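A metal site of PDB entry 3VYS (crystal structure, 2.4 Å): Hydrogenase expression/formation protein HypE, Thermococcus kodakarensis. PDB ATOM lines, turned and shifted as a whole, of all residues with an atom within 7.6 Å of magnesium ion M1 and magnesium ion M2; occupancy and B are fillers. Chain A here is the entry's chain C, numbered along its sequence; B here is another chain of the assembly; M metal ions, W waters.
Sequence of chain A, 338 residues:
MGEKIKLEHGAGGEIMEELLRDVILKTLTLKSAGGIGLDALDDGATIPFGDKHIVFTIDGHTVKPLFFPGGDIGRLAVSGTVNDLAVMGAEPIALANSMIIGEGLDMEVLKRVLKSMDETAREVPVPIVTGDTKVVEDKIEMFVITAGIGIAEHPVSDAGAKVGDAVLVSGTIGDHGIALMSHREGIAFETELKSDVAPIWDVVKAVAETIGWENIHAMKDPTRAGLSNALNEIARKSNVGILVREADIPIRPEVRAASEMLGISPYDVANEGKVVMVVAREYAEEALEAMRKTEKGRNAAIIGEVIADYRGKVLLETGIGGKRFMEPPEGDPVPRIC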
ATOM      1  N   LEU A  41      10.119 -16.222  16.898  1.00  0.00           N
ATOM      2  CA  LEU A  41      11.390 -16.831  16.512  1.00  0.00           C
ATOM      3  C   LEU A  41      11.157 -18.160  15.826  1.00  0.00           C
ATOM      4  O   LEU A  41      11.939 -19.091  15.989  1.00  0.00           O
ATOM      5  CB  LEU A  41      12.294 -17.047  17.726  1.00  0.00           C
ATOM      6  CG  LEU A  41      12.908 -15.786  18.349  1.00  0.00           C
ATOM      7  CD1 LEU A  41      13.688 -16.175  19.585  1.00  0.00           C
ATOM      8  CD2 LEU A  41      13.801 -15.090  17.313  1.00  0.00           C
ATOM      9  N   ASP A  42      10.063 -18.248  15.075  1.00  0.00           N
ATOM     10  CA  ASP A  42       9.735 -19.470  14.367  1.00  0.00           C
ATOM     11  C   ASP A  42      10.572 -19.540  13.091  1.00  0.00           C
ATOM     12  O   ASP A  42      11.268 -18.585  12.731  1.00  0.00           O
ATOM     13  CB  ASP A  42       8.252 -19.495  14.008  1.00  0.00           C
ATOM     14  CG  ASP A  42       7.655 -20.890  14.105  1.00  0.00           C
ATOM     15  OD1 ASP A  42       7.009 -21.195  15.140  1.00  0.00           O
ATOM     16  OD2 ASP A  42       7.835 -21.682  13.160  1.00  0.00           O
ATOM     17  N   ASP A  43      10.479 -20.684  12.405  1.00  0.00           N
ATOM     18  CA  ASP A  43      11.209 -20.910  11.165  1.00  0.00           C
ATOM     19  C   ASP A  43      10.856 -19.862  10.127  1.00  0.00           C
ATOM     20  O   ASP A  43      11.575 -19.683   9.135  1.00  0.00           O
ATOM     21  CB  ASP A  43      10.891 -22.312  10.651  1.00  0.00           C
ATOM     22  CG  ASP A  43      11.367 -23.401  11.587  1.00  0.00           C
ATOM     23  OD1 ASP A  43      12.570 -23.712  11.589  1.00  0.00           O
ATOM     24  OD2 ASP A  43      10.530 -23.936  12.350  1.00  0.00           O
ATOM     25  N   GLY A  44       9.757 -19.166  10.362  1.00  0.00           N
ATOM     26  CA  GLY A  44       9.322 -18.134   9.451  1.00  0.00           C
ATOM     27  C   GLY A  44       8.153 -17.379  10.064  1.00  0.00           C
ATOM     28  O   GLY A  44       7.695 -17.731  11.150  1.00  0.00           O
ATOM     29  N   THR A  57      10.165 -15.958   5.037  1.00  0.00           N
ATOM     30  CA  THR A  57      11.344 -16.364   5.743  1.00  0.00           C
ATOM     31  C   THR A  57      12.593 -15.946   4.998  1.00  0.00           C
ATOM     32  O   THR A  57      12.567 -15.753   3.777  1.00  0.00           O
ATOM     33  CB  THR A  57      11.369 -17.875   5.933  1.00  0.00           C
ATOM     34  OG1 THR A  57      12.446 -18.234   6.795  1.00  0.00           O
ATOM     35  CG2 THR A  57      11.540 -18.567   4.590  1.00  0.00           C
ATOM     36  N   ILE A  58      13.696 -15.795   5.732  1.00  0.00           N
ATOM     37  CA  ILE A  58      14.971 -15.419   5.144  1.00  0.00           C
ATOM     38  C   ILE A  58      16.073 -16.157   5.902  1.00  0.00           C
ATOM     39  O   ILE A  58      15.937 -16.434   7.093  1.00  0.00           O
ATOM     40  CB  ILE A  58      15.192 -13.885   5.223  1.00  0.00           C
ATOM     41  CG1 ILE A  58      16.366 -13.496   4.337  1.00  0.00           C
ATOM     42  CG2 ILE A  58      15.430 -13.453   6.666  1.00  0.00           C
ATOM     43  CD1 ILE A  58      16.538 -12.015   4.139  1.00  0.00           C
ATOM     44  N   ASP A  59      17.155 -16.486   5.198  1.00  0.00           N
ATOM     45  CA  ASP A  59      18.258 -17.197   5.828  1.00  0.00           C
ATOM     46  C   ASP A  59      19.628 -16.861   5.236  1.00  0.00           C
ATOM     47  O   ASP A  59      19.807 -16.811   4.012  1.00  0.00           O
ATOM     48  CB  ASP A  59      18.039 -18.714   5.724  1.00  0.00           C
ATOM     49  CG  ASP A  59      18.313 -19.429   7.025  1.00  0.00           C
ATOM     50  OD1 ASP A  59      19.310 -19.091   7.706  1.00  0.00           O
ATOM     51  OD2 ASP A  59      17.546 -20.353   7.372  1.00  0.00           O
ATOM     52  N   GLY A  60      20.588 -16.612   6.108  1.00  0.00           N
ATOM     53  CA  GLY A  60      21.926 -16.309   5.662  1.00  0.00           C
ATOM     54  C   GLY A  60      22.761 -17.570   5.659  1.00  0.00           C
ATOM     55  O   GLY A  60      22.645 -18.403   6.557  1.00  0.00           O
ATOM     56  N   HIS A  61      23.590 -17.736   4.646  1.00  0.00           N
ATOM     57  CA  HIS A  61      24.456 -18.908   4.538  1.00  0.00           C
ATOM     58  C   HIS A  61      25.884 -18.460   4.390  1.00  0.00           C
ATOM     59  O   HIS A  61      26.207 -17.625   3.530  1.00  0.00           O
ATOM     60  CB  HIS A  61      24.009 -19.765   3.372  1.00  0.00           C
ATOM     61  CG  HIS A  61      22.623 -20.294   3.542  1.00  0.00           C
ATOM     62  ND1 HIS A  61      22.307 -21.295   4.432  1.00  0.00           N
ATOM     63  CD2 HIS A  61      21.443 -19.877   3.015  1.00  0.00           C
ATOM     64  CE1 HIS A  61      21.003 -21.473   4.454  1.00  0.00           C
ATOM     65  NE2 HIS A  61      20.447 -20.622   3.610  1.00  0.00           N
ATOM     66  N   GLY A  80      17.684 -24.707   2.534  1.00  0.00           N
ATOM     67  CA  GLY A  80      17.339 -24.075   3.790  1.00  0.00           C
ATOM     68  C   GLY A  80      16.062 -23.246   3.764  1.00  0.00           C
ATOM     69  O   GLY A  80      15.218 -23.380   4.637  1.00  0.00           O
ATOM     70  N   THR A  81      15.921 -22.400   2.757  1.00  0.00           N
ATOM     71  CA  THR A  81      14.726 -21.565   2.673  1.00  0.00           C
ATOM     72  C   THR A  81      13.470 -22.386   2.393  1.00  0.00           C
ATOM     73  O   THR A  81      12.433 -22.152   2.998  1.00  0.00           O
ATOM     74  CB  THR A  81      14.894 -20.481   1.602  1.00  0.00           C
ATOM     75  OG1 THR A  81      16.072 -19.712   1.883  1.00  0.00           O
ATOM     76  CG2 THR A  81      13.677 -19.551   1.606  1.00  0.00           C
ATOM     77  N   ASN A  83      13.010 -25.486   3.172  1.00  0.00           N
ATOM     78  CA  ASN A  83      12.686 -26.252   4.363  1.00  0.00           C
ATOM     79  C   ASN A  83      12.022 -25.387   5.423  1.00  0.00           C
ATOM     80  O   ASN A  83      11.078 -25.834   6.063  1.00  0.00           O
ATOM     81  CB  ASN A  83      13.923 -26.957   4.914  1.00  0.00           C
ATOM     82  CG  ASN A  83      14.385 -28.095   4.017  1.00  0.00           C
ATOM     83  OD1 ASN A  83      13.693 -28.465   3.055  1.00  0.00           O
ATOM     84  ND2 ASN A  83      15.542 -28.667   4.333  1.00  0.00           N
ATOM     85  N   ASP A  84      12.502 -24.169   5.605  1.00  0.00           N
ATOM     86  CA  ASP A  84      11.889 -23.286   6.599  1.00  0.00           C
ATOM     87  C   ASP A  84      10.443 -22.957   6.235  1.00  0.00           C
ATOM     88  O   ASP A  84       9.615 -22.778   7.123  1.00  0.00           O
ATOM     89  CB  ASP A  84      12.705 -21.994   6.751  1.00  0.00           C
ATOM     90  CG  ASP A  84      13.766 -22.091   7.834  1.00  0.00           C
ATOM     91  OD1 ASP A  84      13.494 -22.694   8.889  1.00  0.00           O
ATOM     92  OD2 ASP A  84      14.881 -21.557   7.634  1.00  0.00           O
ATOM     93  N   LEU A  85      10.140 -22.860   4.950  1.00  0.00           N
ATOM     94  CA  LEU A  85       8.766 -22.587   4.544  1.00  0.00           C
ATOM     95  C   LEU A  85       7.943 -23.848   4.831  1.00  0.00           C
ATOM     96  O   LEU A  85       6.844 -23.777   5.387  1.00  0.00           O
ATOM     97  CB  LEU A  85       8.697 -22.265   3.052  1.00  0.00           C
ATOM     98  CG  LEU A  85       9.210 -20.894   2.571  1.00  0.00           C
ATOM     99  CD1 LEU A  85       9.403 -20.931   1.066  1.00  0.00           C
ATOM    100  CD2 LEU A  85       8.218 -19.797   2.967  1.00  0.00           C
ATOM    101  N   VAL A  87       8.347 -26.372   7.071  1.00  0.00           N
ATOM    102  CA  VAL A  87       8.038 -26.692   8.457  1.00  0.00           C
ATOM    103  C   VAL A  87       6.976 -25.747   9.020  1.00  0.00           C
ATOM    104  O   VAL A  87       6.499 -25.921  10.144  1.00  0.00           O
ATOM    105  CB  VAL A  87       9.311 -26.659   9.374  1.00  0.00           C
ATOM    106  CG1 VAL A  87      10.257 -27.782   8.966  1.00  0.00           C
ATOM    107  CG2 VAL A  87      10.017 -25.320   9.264  1.00  0.00           C
ATOM    108  N   MET A  88       6.604 -24.749   8.228  1.00  0.00           N
ATOM    109  CA  MET A  88       5.569 -23.803   8.636  1.00  0.00           C
ATOM    110  C   MET A  88       4.257 -24.316   8.087  1.00  0.00           C
ATOM    111  O   MET A  88       3.187 -23.867   8.495  1.00  0.00           O
ATOM    112  CB  MET A  88       5.851 -22.405   8.071  1.00  0.00           C
ATOM    113  CG  MET A  88       7.033 -21.675   8.696  1.00  0.00           C
ATOM    114  SD  MET A  88       6.954 -21.652  10.488  1.00  0.00           S
ATOM    115  CE  MET A  88       5.945 -20.168  10.762  1.00  0.00           C
ATOM    116  N   ASP A 158       5.826 -23.647  16.350  1.00  0.00           N
ATOM    117  CA  ASP A 158       6.586 -24.408  17.332  1.00  0.00           C
ATOM    118  C   ASP A 158       5.846 -24.534  18.655  1.00  0.00           C
ATOM    119  O   ASP A 158       6.326 -25.203  19.569  1.00  0.00           O
ATOM    120  CB  ASP A 158       7.934 -23.721  17.602  1.00  0.00           C
ATOM    121  CG  ASP A 158       8.702 -23.418  16.334  1.00  0.00           C
ATOM    122  OD1 ASP A 158       8.379 -23.992  15.273  1.00  0.00           O
ATOM    123  OD2 ASP A 158       9.638 -22.604  16.410  1.00  0.00           O
ATOM    124  N   MET A 219       6.431 -28.460  13.817  1.00  0.00           N
ATOM    125  CA  MET A 219       7.552 -28.843  12.969  1.00  0.00           C
ATOM    126  C   MET A 219       8.719 -27.890  13.122  1.00  0.00           C
ATOM    127  O   MET A 219       8.580 -26.781  13.631  1.00  0.00           O
ATOM    128  CB  MET A 219       7.148 -28.875  11.506  1.00  0.00           C
ATOM    129  CG  MET A 219       6.264 -30.029  11.098  1.00  0.00           C
ATOM    130  SD  MET A 219       5.978 -29.990   9.330  1.00  0.00           S
ATOM    131  CE  MET A 219       4.898 -28.573   9.216  1.00  0.00           C
ATOM    132  N   LYS A 220       9.881 -28.339  12.651  1.00  0.00           N
ATOM    133  CA  LYS A 220      11.097 -27.540  12.701  1.00  0.00           C
ATOM    134  C   LYS A 220      12.258 -28.312  12.074  1.00  0.00           C
ATOM    135  O   LYS A 220      12.478 -29.496  12.359  1.00  0.00           O
ATOM    136  CB  LYS A 220      11.440 -27.155  14.135  1.00  0.00           C
ATOM    137  CG  LYS A 220      12.746 -26.395  14.267  1.00  0.00           C
ATOM    138  CD  LYS A 220      12.779 -25.609  15.566  1.00  0.00           C
ATOM    139  CE  LYS A 220      11.784 -24.445  15.541  1.00  0.00           C
ATOM    140  NZ  LYS A 220      12.163 -23.350  14.602  1.00  0.00           N
ATOM    141  N   ASP A 221      13.003 -27.643  11.198  1.00  0.00           N
ATOM    142  CA  ASP A 221      14.144 -28.259  10.570  1.00  0.00           C
ATOM    143  C   ASP A 221      15.280 -28.040  11.553  1.00  0.00           C
ATOM    144  O   ASP A 221      15.643 -26.905  11.860  1.00  0.00           O
ATOM    145  CB  ASP A 221      14.428 -27.621   9.197  1.00  0.00           C
ATOM    146  CG  ASP A 221      14.572 -26.120   9.267  1.00  0.00           C
ATOM    147  OD1 ASP A 221      13.909 -25.500  10.130  1.00  0.00           O
ATOM    148  OD2 ASP A 221      15.333 -25.554   8.456  1.00  0.00           O
ATOM    149  N   PRO A 222      15.864 -29.121  12.042  1.00  0.00           N
ATOM    150  CA  PRO A 222      16.888 -29.000  13.065  1.00  0.00           C
ATOM    151  C   PRO A 222      18.226 -28.680  12.434  1.00  0.00           C
ATOM    152  O   PRO A 222      19.040 -29.551  12.212  1.00  0.00           O
ATOM    153  CB  PRO A 222      16.921 -30.389  13.687  1.00  0.00           C
ATOM    154  CG  PRO A 222      16.458 -31.285  12.627  1.00  0.00           C
ATOM    155  CD  PRO A 222      15.448 -30.518  11.851  1.00  0.00           C
ATOM    156  N   THR A 223      18.440 -27.393  12.189  1.00  0.00           N
ATOM    157  CA  THR A 223      19.654 -26.932  11.568  1.00  0.00           C
ATOM    158  C   THR A 223      20.674 -26.539  12.624  1.00  0.00           C
ATOM    159  O   THR A 223      21.171 -27.382  13.332  1.00  0.00           O
ATOM    160  CB  THR A 223      19.384 -25.746  10.639  1.00  0.00           C
ATOM    161  OG1 THR A 223      18.584 -24.789  11.329  1.00  0.00           O
ATOM    162  CG2 THR A 223      18.621 -26.215   9.425  1.00  0.00           C
ATOM    163  N   ARG A 224      20.976 -25.258  12.755  1.00  0.00           N
ATOM    164  CA  ARG A 224      22.015 -24.885  13.700  1.00  0.00           C
ATOM    165  C   ARG A 224      21.673 -25.347  15.104  1.00  0.00           C
ATOM    166  O   ARG A 224      20.576 -25.144  15.594  1.00  0.00           O
ATOM    167  CB  ARG A 224      22.222 -23.373  13.700  1.00  0.00           C
ATOM    168  CG  ARG A 224      23.289 -22.879  12.739  1.00  0.00           C
ATOM    169  CD  ARG A 224      23.552 -21.405  12.953  1.00  0.00           C
ATOM    170  NE  ARG A 224      22.363 -20.606  12.672  1.00  0.00           N
ATOM    171  CZ  ARG A 224      22.296 -19.300  12.861  1.00  0.00           C
ATOM    172  NH1 ARG A 224      23.337 -18.639  13.333  1.00  0.00           N
ATOM    173  NH2 ARG A 224      21.177 -18.640  12.588  1.00  0.00           N
ATOM    174  N   GLU A 233      13.416 -26.059  21.581  1.00  0.00           N
ATOM    175  CA  GLU A 233      12.650 -24.892  21.168  1.00  0.00           C
ATOM    176  C   GLU A 233      11.165 -25.209  21.180  1.00  0.00           C
ATOM    177  O   GLU A 233      10.372 -24.418  21.667  1.00  0.00           O
ATOM    178  CB  GLU A 233      13.081 -24.423  19.779  1.00  0.00           C
ATOM    179  CG  GLU A 233      13.688 -23.021  19.800  1.00  0.00           C
ATOM    180  CD  GLU A 233      14.096 -22.524  18.416  1.00  0.00           C
ATOM    181  OE1 GLU A 233      15.018 -23.108  17.807  1.00  0.00           O
ATOM    182  OE2 GLU A 233      13.485 -21.534  17.946  1.00  0.00           O
ATOM    183  N   GLU A 272      20.807 -30.642   7.471  1.00  0.00           N
ATOM    184  CA  GLU A 272      20.321 -29.793   6.399  1.00  0.00           C
ATOM    185  C   GLU A 272      19.295 -30.466   5.501  1.00  0.00           C
ATOM    186  O   GLU A 272      18.830 -29.884   4.539  1.00  0.00           O
ATOM    187  CB  GLU A 272      21.489 -29.224   5.590  1.00  0.00           C
ATOM    188  CG  GLU A 272      22.382 -28.320   6.401  1.00  0.00           C
ATOM    189  CD  GLU A 272      21.631 -27.115   6.940  1.00  0.00           C
ATOM    190  OE1 GLU A 272      20.570 -26.781   6.406  1.00  0.00           O
ATOM    191  OE2 GLU A 272      22.123 -26.496   7.894  1.00  0.00           O
ATOM    192  N   GLY B 131      13.713 -12.875  10.682  1.00  0.00           N
ATOM    193  CA  GLY B 131      15.105 -12.529  10.494  1.00  0.00           C
ATOM    194  C   GLY B 131      16.073 -13.690  10.616  1.00  0.00           C
ATOM    195  O   GLY B 131      15.659 -14.854  10.677  1.00  0.00           O
ATOM    196  N   ASP B 132      17.361 -13.363  10.623  1.00  0.00           N
ATOM    197  CA  ASP B 132      18.419 -14.362  10.747  1.00  0.00           C
ATOM    198  C   ASP B 132      19.700 -13.652  11.161  1.00  0.00           C
ATOM    199  O   ASP B 132      19.925 -12.495  10.788  1.00  0.00           O
ATOM    200  CB  ASP B 132      18.641 -15.079   9.418  1.00  0.00           C
ATOM    201  CG  ASP B 132      19.648 -16.210   9.541  1.00  0.00           C
ATOM    202  OD1 ASP B 132      19.448 -17.087  10.410  1.00  0.00           O
ATOM    203  OD2 ASP B 132      20.629 -16.240   8.766  1.00  0.00           O
ATOM    204  N   LYS B 134      23.964 -14.287  11.541  1.00  0.00           N
ATOM    205  CA  LYS B 134      25.171 -15.076  11.364  1.00  0.00           C
ATOM    206  C   LYS B 134      26.356 -14.272  11.882  1.00  0.00           C
ATOM    207  O   LYS B 134      26.331 -13.038  11.865  1.00  0.00           O
ATOM    208  CB  LYS B 134      25.379 -15.402   9.891  1.00  0.00           C
ATOM    209  CG  LYS B 134      24.421 -16.448   9.341  1.00  0.00           C
ATOM    210  CD  LYS B 134      24.638 -17.807  10.006  1.00  0.00           C
ATOM    211  CE  LYS B 134      23.802 -18.895   9.355  1.00  0.00           C
ATOM    212  NZ  LYS B 134      22.331 -18.647   9.461  1.00  0.00           N
HETATM  213 MG    MG M   1      14.290 -23.260  10.691  1.00  0.00          MG
HETATM  214 MG    MG M   2      16.865 -21.994   8.935  1.00  0.00          MG
HETATM  215 MG    MG M   3       7.921 -24.385  13.030  1.00  0.00          MG
HETATM  216  O   HOH W   1      17.347 -19.015  10.130  1.00  0.00           O
HETATM  217  O   HOH W   2      19.301 -21.595  10.501  1.00  0.00           O
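The side-chain amino group (NZ) of Lys 220 lies within salt-bridge range of the side-chain carboxylate (OD2) of Asp 43 (2.8 Å).
OG1 of Thr 57 is in hydrogen-bond range of O of Asp 43.
OD1 of Asp 59 lies within salt-bridge range of NZ of Lys 134 of chain B (3.5 Å).
Within 4 Å of magnesium ion M1: Asp 43, Asp 84 and Asp 221.
The nearest printed residue that does not touch magnesium ion M1 is Lys 220 (4.5 Å).
Three residues have an atom within 4 Å of magnesium ion M2: Asp 59, Asp 84 and Asp 221.
The nearest printed residue that does not touch magnesium ion M2 is Thr 223 (4.1 Å).
Magnesium ion M1 is bound by OD1 of Asp 43 (2.0 Å), OD1 of Asp 84 (2.0 Å) and OD1 of Asp 221 (2.3 Å).
Magnesium ion M2 is bound by the side-chain carboxylate of Asp 59 and the side-chain carboxylate of Asp 84.
Magnesium ion M2 has two donor atoms within binding distance.
Water W1 bridges the side-chain carboxylate (OD1) of Asp 132 of chain B and the side-chain carboxylate (OD1) of Asp 59.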
